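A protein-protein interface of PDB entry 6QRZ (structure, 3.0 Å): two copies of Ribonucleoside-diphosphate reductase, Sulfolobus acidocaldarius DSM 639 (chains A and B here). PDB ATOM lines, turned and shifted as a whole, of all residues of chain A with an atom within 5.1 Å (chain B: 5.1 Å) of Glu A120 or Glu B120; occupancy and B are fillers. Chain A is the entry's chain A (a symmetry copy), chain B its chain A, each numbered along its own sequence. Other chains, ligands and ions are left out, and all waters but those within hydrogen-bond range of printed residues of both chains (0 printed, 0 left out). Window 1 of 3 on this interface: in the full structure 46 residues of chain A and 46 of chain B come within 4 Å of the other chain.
Among the printed residues, pairs that only touch across the chains: Glu A120 with Ala B127, Gln A121 with Phe B124, Phe A124 with Gln B121, Phe A124 with Phe B124 and Ala A127 with Glu B120.
Glu A120 touches its own counterpart, Glu B120.
Glu A120 touches Ala B123, and with the chains exchanged Ala A123 touches Glu B120.
Glu A120 touches Phe B124, and with the chains exchanged Phe A124 touches Glu B120.
Glu A120 touches Ala B127, and with the chains exchanged Ala A127 touches Glu B120.
Tyr A118 touches none of the printed residues of chain B.
Glu A120 touches four residues of chain B.
Of the printed residues of chain B, Phe A124 touches Glu B120, Gln B121 and Phe B124.
Glu B120 touches just these residues of chain A: Glu A120 (2.7 Å), Ala A123 (3.0 Å), Phe A124 (2.6 Å) and Ala A127 (3.6 Å).
Printed residues of chain A within 4 Å of Ala B123: Glu A120 (3.0 Å).
Printed residues of chain A within 4 Å of Phe B124: Glu A120 (2.6 Å), Gln A121 (3.4 Å) and Phe A124 (3.4 Å).
Printed residues of chain A within 4 Å of Ala B127: Glu A120 (3.6 Å).
The side-chain carboxylate of Glu A120 sits close to the backbone carbonyl oxygen of Glu B120 (2.7 Å).
The side-chain carboxylate (OE2) of Glu A120 lies close to the backbone NH (N) of Phe B124, at 2.6 Å.
The backbone NH of Phe A124 lies close to the side-chain carboxylate of Glu B120, at 2.6 Å.
The side-chain carboxylate of Glu A120 lies close to the backbone carbonyl oxygen of Ala B123 (3.0 Å).
O of Ala A123 sits close to OE1 of Glu B120 (3.0 Å).
Of the 13 printed residues of chain B, 5 touch a printed residue of chain A.
Printed residues of chain B that touch a printed residue of chain A: Glu B120, Gln B121, Ala B123, Phe B124 and Ala B127.
Printed residues of chain A that touch a printed residue of chain B: Glu A120, Gln A121, Ala A123, Phe A124 and Ala A127.
Among the printed residues, 10 pairs touch across the chains.
Among the printed residues, no Asp or Glu carboxylate lies within 4 Å of a Lys or Arg side-chain nitrogen of the other chain.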
ATOM      1  N   ALA A  97     -18.865 -19.446  25.136  1.00  0.00           N
ATOM      2  CA  ALA A  97     -18.144 -18.383  25.821  1.00  0.00           C
ATOM      3  C   ALA A  97     -16.637 -18.479  25.626  1.00  0.00           C
ATOM      4  O   ALA A  97     -15.937 -17.476  25.808  1.00  0.00           O
ATOM      5  CB  ALA A  97     -18.473 -18.398  27.315  1.00  0.00           C
ATOM      6  N   ILE A 104     -13.578 -12.698  18.176  1.00  0.00           N
ATOM      7  CA  ILE A 104     -13.188 -11.382  18.672  1.00  0.00           C
ATOM      8  C   ILE A 104     -11.832 -10.981  18.104  1.00  0.00           C
ATOM      9  O   ILE A 104     -11.644  -9.845  17.653  1.00  0.00           O
ATOM     10  CB  ILE A 104     -13.186 -11.367  20.211  1.00  0.00           C
ATOM     11  CG1 ILE A 104     -14.594 -11.632  20.748  1.00  0.00           C
ATOM     12  CG2 ILE A 104     -12.665 -10.038  20.731  1.00  0.00           C
ATOM     13  CD1 ILE A 104     -14.670 -11.698  22.257  1.00  0.00           C
ATOM     14  N   ASP A 115     -17.708  -4.038  16.444  1.00  0.00           N
ATOM     15  CA  ASP A 115     -18.018  -5.456  16.583  1.00  0.00           C
ATOM     16  C   ASP A 115     -17.275  -6.066  17.763  1.00  0.00           C
ATOM     17  O   ASP A 115     -17.811  -6.940  18.453  1.00  0.00           O
ATOM     18  CB  ASP A 115     -17.680  -6.198  15.291  1.00  0.00           C
ATOM     19  CG  ASP A 115     -18.675  -5.920  14.183  1.00  0.00           C
ATOM     20  OD1 ASP A 115     -19.854  -5.651  14.494  1.00  0.00           O
ATOM     21  OD2 ASP A 115     -18.281  -5.973  13.001  1.00  0.00           O
ATOM     22  N   VAL A 116     -16.042  -5.618  18.009  1.00  0.00           N
ATOM     23  CA  VAL A 116     -15.293  -6.102  19.166  1.00  0.00           C
ATOM     24  C   VAL A 116     -16.001  -5.711  20.457  1.00  0.00           C
ATOM     25  O   VAL A 116     -16.029  -6.481  21.423  1.00  0.00           O
ATOM     26  CB  VAL A 116     -13.846  -5.574  19.132  1.00  0.00           C
ATOM     27  CG1 VAL A 116     -13.095  -5.986  20.389  1.00  0.00           C
ATOM     28  CG2 VAL A 116     -13.125  -6.080  17.896  1.00  0.00           C
ATOM     29  N   ILE A 117     -16.596  -4.517  20.490  1.00  0.00           N
ATOM     30  CA  ILE A 117     -17.266  -4.057  21.702  1.00  0.00           C
ATOM     31  C   ILE A 117     -18.477  -4.927  22.013  1.00  0.00           C
ATOM     32  O   ILE A 117     -18.708  -5.298  23.170  1.00  0.00           O
ATOM     33  CB  ILE A 117     -17.651  -2.572  21.570  1.00  0.00           C
ATOM     34  CG1 ILE A 117     -16.397  -1.699  21.531  1.00  0.00           C
ATOM     35  CG2 ILE A 117     -18.547  -2.147  22.721  1.00  0.00           C
ATOM     36  CD1 ILE A 117     -16.684  -0.236  21.280  1.00  0.00           C
ATOM     37  N   TYR A 118     -19.268  -5.274  20.994  1.00  0.00           N
ATOM     38  CA  TYR A 118     -20.432  -6.117  21.246  1.00  0.00           C
ATOM     39  C   TYR A 118     -20.036  -7.577  21.428  1.00  0.00           C
ATOM     40  O   TYR A 118     -20.475  -8.227  22.382  1.00  0.00           O
ATOM     41  CB  TYR A 118     -21.458  -5.990  20.121  1.00  0.00           C
ATOM     42  CG  TYR A 118     -22.687  -6.836  20.373  1.00  0.00           C
ATOM     43  CD1 TYR A 118     -23.685  -6.403  21.236  1.00  0.00           C
ATOM     44  CD2 TYR A 118     -22.840  -8.078  19.769  1.00  0.00           C
ATOM     45  CE1 TYR A 118     -24.804  -7.175  21.482  1.00  0.00           C
ATOM     46  CE2 TYR A 118     -23.956  -8.857  20.010  1.00  0.00           C
ATOM     47  CZ  TYR A 118     -24.936  -8.399  20.865  1.00  0.00           C
ATOM     48  OH  TYR A 118     -26.050  -9.172  21.105  1.00  0.00           O
ATOM     49  N   LEU A 119     -19.214  -8.112  20.518  1.00  0.00           N
ATOM     50  CA  LEU A 119     -18.778  -9.501  20.639  1.00  0.00           C
ATOM     51  C   LEU A 119     -18.105  -9.763  21.977  1.00  0.00           C
ATOM     52  O   LEU A 119     -18.115 -10.898  22.466  1.00  0.00           O
ATOM     53  CB  LEU A 119     -17.828  -9.863  19.499  1.00  0.00           C
ATOM     54  CG  LEU A 119     -18.502 -10.265  18.191  1.00  0.00           C
ATOM     55  CD1 LEU A 119     -17.471 -10.428  17.094  1.00  0.00           C
ATOM     56  CD2 LEU A 119     -19.284 -11.552  18.391  1.00  0.00           C
ATOM     57  N   GLU A 120     -17.517  -8.733  22.577  1.00  0.00           N
ATOM     58  CA  GLU A 120     -16.959  -8.878  23.911  1.00  0.00           C
ATOM     59  C   GLU A 120     -18.044  -8.824  24.982  1.00  0.00           C
ATOM     60  O   GLU A 120     -17.898  -9.450  26.036  1.00  0.00           O
ATOM     61  CB  GLU A 120     -15.892  -7.807  24.135  1.00  0.00           C
ATOM     62  CG  GLU A 120     -15.052  -8.008  25.361  1.00  0.00           C
ATOM     63  CD  GLU A 120     -15.734  -7.472  26.583  1.00  0.00           C
ATOM     64  OE1 GLU A 120     -16.258  -6.342  26.507  1.00  0.00           O
ATOM     65  OE2 GLU A 120     -15.773  -8.191  27.600  1.00  0.00           O
ATOM     66  N   GLN A 121     -19.135  -8.091  24.737  1.00  0.00           N
ATOM     67  CA  GLN A 121     -20.306  -8.218  25.601  1.00  0.00           C
ATOM     68  C   GLN A 121     -21.120  -9.452  25.241  1.00  0.00           C
ATOM     69  O   GLN A 121     -21.667 -10.122  26.126  1.00  0.00           O
ATOM     70  CB  GLN A 121     -21.196  -6.980  25.502  1.00  0.00           C
ATOM     71  CG  GLN A 121     -22.518  -7.148  26.246  1.00  0.00           C
ATOM     72  CD  GLN A 121     -23.580  -6.162  25.817  1.00  0.00           C
ATOM     73  OE1 GLN A 121     -23.577  -5.680  24.685  1.00  0.00           O
ATOM     74  NE2 GLN A 121     -24.505  -5.859  26.720  1.00  0.00           N
ATOM     75  N   PHE A 122     -21.209  -9.760  23.946  1.00  0.00           N
ATOM     76  CA  PHE A 122     -21.989 -10.902  23.486  1.00  0.00           C
ATOM     77  C   PHE A 122     -21.544 -12.197  24.154  1.00  0.00           C
ATOM     78  O   PHE A 122     -22.335 -13.140  24.269  1.00  0.00           O
ATOM     79  CB  PHE A 122     -21.884 -11.002  21.963  1.00  0.00           C
ATOM     80  CG  PHE A 122     -22.289 -12.330  21.408  1.00  0.00           C
ATOM     81  CD1 PHE A 122     -23.616 -12.718  21.388  1.00  0.00           C
ATOM     82  CD2 PHE A 122     -21.339 -13.186  20.888  1.00  0.00           C
ATOM     83  CE1 PHE A 122     -23.980 -13.942  20.869  1.00  0.00           C
ATOM     84  CE2 PHE A 122     -21.698 -14.399  20.370  1.00  0.00           C
ATOM     85  CZ  PHE A 122     -23.019 -14.781  20.359  1.00  0.00           C
ATOM     86  N   ALA A 123     -20.291 -12.259  24.607  1.00  0.00           N
ATOM     87  CA  ALA A 123     -19.819 -13.373  25.415  1.00  0.00           C
ATOM     88  C   ALA A 123     -20.094 -13.182  26.902  1.00  0.00           C
ATOM     89  O   ALA A 123     -20.164 -14.173  27.637  1.00  0.00           O
ATOM     90  CB  ALA A 123     -18.319 -13.582  25.196  1.00  0.00           C
ATOM     91  N   PHE A 124     -20.246 -11.935  27.360  1.00  0.00           N
ATOM     92  CA  PHE A 124     -20.527 -11.695  28.772  1.00  0.00           C
ATOM     93  C   PHE A 124     -21.908 -12.207  29.153  1.00  0.00           C
ATOM     94  O   PHE A 124     -22.101 -12.725  30.258  1.00  0.00           O
ATOM     95  CB  PHE A 124     -20.391 -10.207  29.092  1.00  0.00           C
ATOM     96  CG  PHE A 124     -20.839  -9.845  30.477  1.00  0.00           C
ATOM     97  CD1 PHE A 124     -20.180 -10.346  31.587  1.00  0.00           C
ATOM     98  CD2 PHE A 124     -21.921  -9.003  30.669  1.00  0.00           C
ATOM     99  CE1 PHE A 124     -20.596 -10.018  32.862  1.00  0.00           C
ATOM    100  CE2 PHE A 124     -22.338  -8.669  31.942  1.00  0.00           C
ATOM    101  CZ  PHE A 124     -21.674  -9.176  33.038  1.00  0.00           C
ATOM    102  N   ALA A 127     -21.398 -16.136  29.254  1.00  0.00           N
ATOM    103  CA  ALA A 127     -20.825 -16.578  30.520  1.00  0.00           C
ATOM    104  C   ALA A 127     -21.800 -16.371  31.670  1.00  0.00           C
ATOM    105  O   ALA A 127     -21.798 -17.145  32.634  1.00  0.00           O
ATOM    106  CB  ALA A 127     -19.512 -15.845  30.793  1.00  0.00           C
ATOM    107  N   ALA B  97      -9.259  -3.299  26.050  1.00  0.00           N
ATOM    108  CA  ALA B  97     -10.391  -4.136  25.679  1.00  0.00           C
ATOM    109  C   ALA B  97     -10.088  -5.038  24.491  1.00  0.00           C
ATOM    110  O   ALA B  97     -10.779  -6.045  24.303  1.00  0.00           O
ATOM    111  CB  ALA B  97     -11.611  -3.266  25.368  1.00  0.00           C
ATOM    112  N   ILE B 104      -7.257 -14.069  27.442  1.00  0.00           N
ATOM    113  CA  ILE B 104      -8.404 -14.968  27.525  1.00  0.00           C
ATOM    114  C   ILE B 104      -8.099 -16.285  26.823  1.00  0.00           C
ATOM    115  O   ILE B 104      -8.386 -17.366  27.350  1.00  0.00           O
ATOM    116  CB  ILE B 104      -9.658 -14.291  26.942  1.00  0.00           C
ATOM    117  CG1 ILE B 104     -10.021 -13.049  27.758  1.00  0.00           C
ATOM    118  CG2 ILE B 104     -10.825 -15.264  26.915  1.00  0.00           C
ATOM    119  CD1 ILE B 104     -11.208 -12.286  27.214  1.00  0.00           C
ATOM    120  N   ASP B 115     -11.162 -18.296  35.312  1.00  0.00           N
ATOM    121  CA  ASP B 115     -10.464 -17.092  34.877  1.00  0.00           C
ATOM    122  C   ASP B 115     -11.018 -16.585  33.553  1.00  0.00           C
ATOM    123  O   ASP B 115     -11.098 -15.372  33.332  1.00  0.00           O
ATOM    124  CB  ASP B 115      -8.965 -17.363  34.765  1.00  0.00           C
ATOM    125  CG  ASP B 115      -8.290 -17.466  36.118  1.00  0.00           C
ATOM    126  OD1 ASP B 115      -8.768 -16.819  37.073  1.00  0.00           O
ATOM    127  OD2 ASP B 115      -7.278 -18.187  36.226  1.00  0.00           O
ATOM    128  N   VAL B 116     -11.406 -17.500  32.660  1.00  0.00           N
ATOM    129  CA  VAL B 116     -12.015 -17.094  31.396  1.00  0.00           C
ATOM    130  C   VAL B 116     -13.330 -16.368  31.651  1.00  0.00           C
ATOM    131  O   VAL B 116     -13.663 -15.399  30.961  1.00  0.00           O
ATOM    132  CB  VAL B 116     -12.210 -18.313  30.475  1.00  0.00           C
ATOM    133  CG1 VAL B 116     -12.942 -17.911  29.203  1.00  0.00           C
ATOM    134  CG2 VAL B 116     -10.872 -18.943  30.137  1.00  0.00           C
ATOM    135  N   ILE B 117     -14.090 -16.815  32.654  1.00  0.00           N
ATOM    136  CA  ILE B 117     -15.379 -16.194  32.938  1.00  0.00           C
ATOM    137  C   ILE B 117     -15.194 -14.758  33.411  1.00  0.00           C
ATOM    138  O   ILE B 117     -15.927 -13.854  32.990  1.00  0.00           O
ATOM    139  CB  ILE B 117     -16.164 -17.034  33.962  1.00  0.00           C
ATOM    140  CG1 ILE B 117     -16.568 -18.375  33.353  1.00  0.00           C
ATOM    141  CG2 ILE B 117     -17.397 -16.284  34.438  1.00  0.00           C
ATOM    142  CD1 ILE B 117     -17.237 -19.311  34.333  1.00  0.00           C
ATOM    143  N   TYR B 118     -14.214 -14.515  34.285  1.00  0.00           N
ATOM    144  CA  TYR B 118     -13.995 -13.150  34.754  1.00  0.00           C
ATOM    145  C   TYR B 118     -13.265 -12.312  33.712  1.00  0.00           C
ATOM    146  O   TYR B 118     -13.683 -11.189  33.413  1.00  0.00           O
ATOM    147  CB  TYR B 118     -13.219 -13.140  36.071  1.00  0.00           C
ATOM    148  CG  TYR B 118     -13.002 -11.735  36.591  1.00  0.00           C
ATOM    149  CD1 TYR B 118     -14.013 -11.060  37.263  1.00  0.00           C
ATOM    150  CD2 TYR B 118     -11.796 -11.074  36.392  1.00  0.00           C
ATOM    151  CE1 TYR B 118     -13.826  -9.773  37.730  1.00  0.00           C
ATOM    152  CE2 TYR B 118     -11.602  -9.786  36.855  1.00  0.00           C
ATOM    153  CZ  TYR B 118     -12.619  -9.143  37.526  1.00  0.00           C
ATOM    154  OH  TYR B 118     -12.428  -7.861  37.990  1.00  0.00           O
ATOM    155  N   LEU B 119     -12.167 -12.836  33.156  1.00  0.00           N
ATOM    156  CA  LEU B 119     -11.427 -12.096  32.136  1.00  0.00           C
ATOM    157  C   LEU B 119     -12.316 -11.714  30.964  1.00  0.00           C
ATOM    158  O   LEU B 119     -12.050 -10.721  30.279  1.00  0.00           O
ATOM    159  CB  LEU B 119     -10.236 -12.915  31.642  1.00  0.00           C
ATOM    160  CG  LEU B 119      -8.983 -12.832  32.507  1.00  0.00           C
ATOM    161  CD1 LEU B 119      -7.939 -13.814  32.018  1.00  0.00           C
ATOM    162  CD2 LEU B 119      -8.439 -11.415  32.489  1.00  0.00           C
ATOM    163  N   GLU B 120     -13.370 -12.488  30.719  1.00  0.00           N
ATOM    164  CA  GLU B 120     -14.331 -12.120  29.693  1.00  0.00           C
ATOM    165  C   GLU B 120     -15.294 -11.045  30.187  1.00  0.00           C
ATOM    166  O   GLU B 120     -15.772 -10.235  29.387  1.00  0.00           O
ATOM    167  CB  GLU B 120     -15.075 -13.370  29.222  1.00  0.00           C
ATOM    168  CG  GLU B 120     -15.899 -13.177  27.985  1.00  0.00           C
ATOM    169  CD  GLU B 120     -17.242 -12.596  28.310  1.00  0.00           C
ATOM    170  OE1 GLU B 120     -17.872 -13.089  29.267  1.00  0.00           O
ATOM    171  OE2 GLU B 120     -17.647 -11.633  27.632  1.00  0.00           O
ATOM    172  N   GLN B 121     -15.589 -11.012  31.490  1.00  0.00           N
ATOM    173  CA  GLN B 121     -16.283  -9.857  32.051  1.00  0.00           C
ATOM    174  C   GLN B 121     -15.319  -8.706  32.296  1.00  0.00           C
ATOM    175  O   GLN B 121     -15.676  -7.537  32.102  1.00  0.00           O
ATOM    176  CB  GLN B 121     -16.979 -10.220  33.362  1.00  0.00           C
ATOM    177  CG  GLN B 121     -17.562  -9.000  34.073  1.00  0.00           C
ATOM    178  CD  GLN B 121     -17.854  -9.240  35.537  1.00  0.00           C
ATOM    179  OE1 GLN B 121     -17.220 -10.074  36.181  1.00  0.00           O
ATOM    180  NE2 GLN B 121     -18.817  -8.501  36.075  1.00  0.00           N
ATOM    181  N   PHE B 122     -14.096  -9.023  32.725  1.00  0.00           N
ATOM    182  CA  PHE B 122     -13.102  -7.999  33.022  1.00  0.00           C
ATOM    183  C   PHE B 122     -12.860  -7.083  31.829  1.00  0.00           C
ATOM    184  O   PHE B 122     -12.449  -5.931  32.004  1.00  0.00           O
ATOM    185  CB  PHE B 122     -11.805  -8.673  33.474  1.00  0.00           C
ATOM    186  CG  PHE B 122     -10.604  -7.784  33.421  1.00  0.00           C
ATOM    187  CD1 PHE B 122     -10.440  -6.754  34.329  1.00  0.00           C
ATOM    188  CD2 PHE B 122      -9.627  -7.992  32.468  1.00  0.00           C
ATOM    189  CE1 PHE B 122      -9.326  -5.944  34.276  1.00  0.00           C
ATOM    190  CE2 PHE B 122      -8.519  -7.191  32.415  1.00  0.00           C
ATOM    191  CZ  PHE B 122      -8.366  -6.165  33.318  1.00  0.00           C
ATOM    192  N   ALA B 123     -13.115  -7.571  30.615  1.00  0.00           N
ATOM    193  CA  ALA B 123     -13.091  -6.732  29.427  1.00  0.00           C
ATOM    194  C   ALA B 123     -14.422  -6.037  29.167  1.00  0.00           C
ATOM    195  O   ALA B 123     -14.441  -4.996  28.500  1.00  0.00           O
ATOM    196  CB  ALA B 123     -12.702  -7.565  28.203  1.00  0.00           C
ATOM    197  N   PHE B 124     -15.530  -6.588  29.671  1.00  0.00           N
ATOM    198  CA  PHE B 124     -16.830  -5.956  29.467  1.00  0.00           C
ATOM    199  C   PHE B 124     -16.921  -4.632  30.210  1.00  0.00           C
ATOM    200  O   PHE B 124     -17.523  -3.674  29.713  1.00  0.00           O
ATOM    201  CB  PHE B 124     -17.950  -6.901  29.899  1.00  0.00           C
ATOM    202  CG  PHE B 124     -19.310  -6.266  29.894  1.00  0.00           C
ATOM    203  CD1 PHE B 124     -19.875  -5.816  28.714  1.00  0.00           C
ATOM    204  CD2 PHE B 124     -20.021  -6.118  31.072  1.00  0.00           C
ATOM    205  CE1 PHE B 124     -21.124  -5.226  28.709  1.00  0.00           C
ATOM    206  CE2 PHE B 124     -21.271  -5.533  31.073  1.00  0.00           C
ATOM    207  CZ  PHE B 124     -21.823  -5.088  29.890  1.00  0.00           C
ATOM    208  N   ALA B 127     -14.676  -2.223  28.004  1.00  0.00           N
ATOM    209  CA  ALA B 127     -15.408  -1.693  26.860  1.00  0.00           C
ATOM    210  C   ALA B 127     -16.518  -0.750  27.302  1.00  0.00           C
ATOM    211  O   ALA B 127     -16.846   0.204  26.587  1.00  0.00           O
ATOM    212  CB  ALA B 127     -15.979  -2.835  26.021  1.00  0.00           C
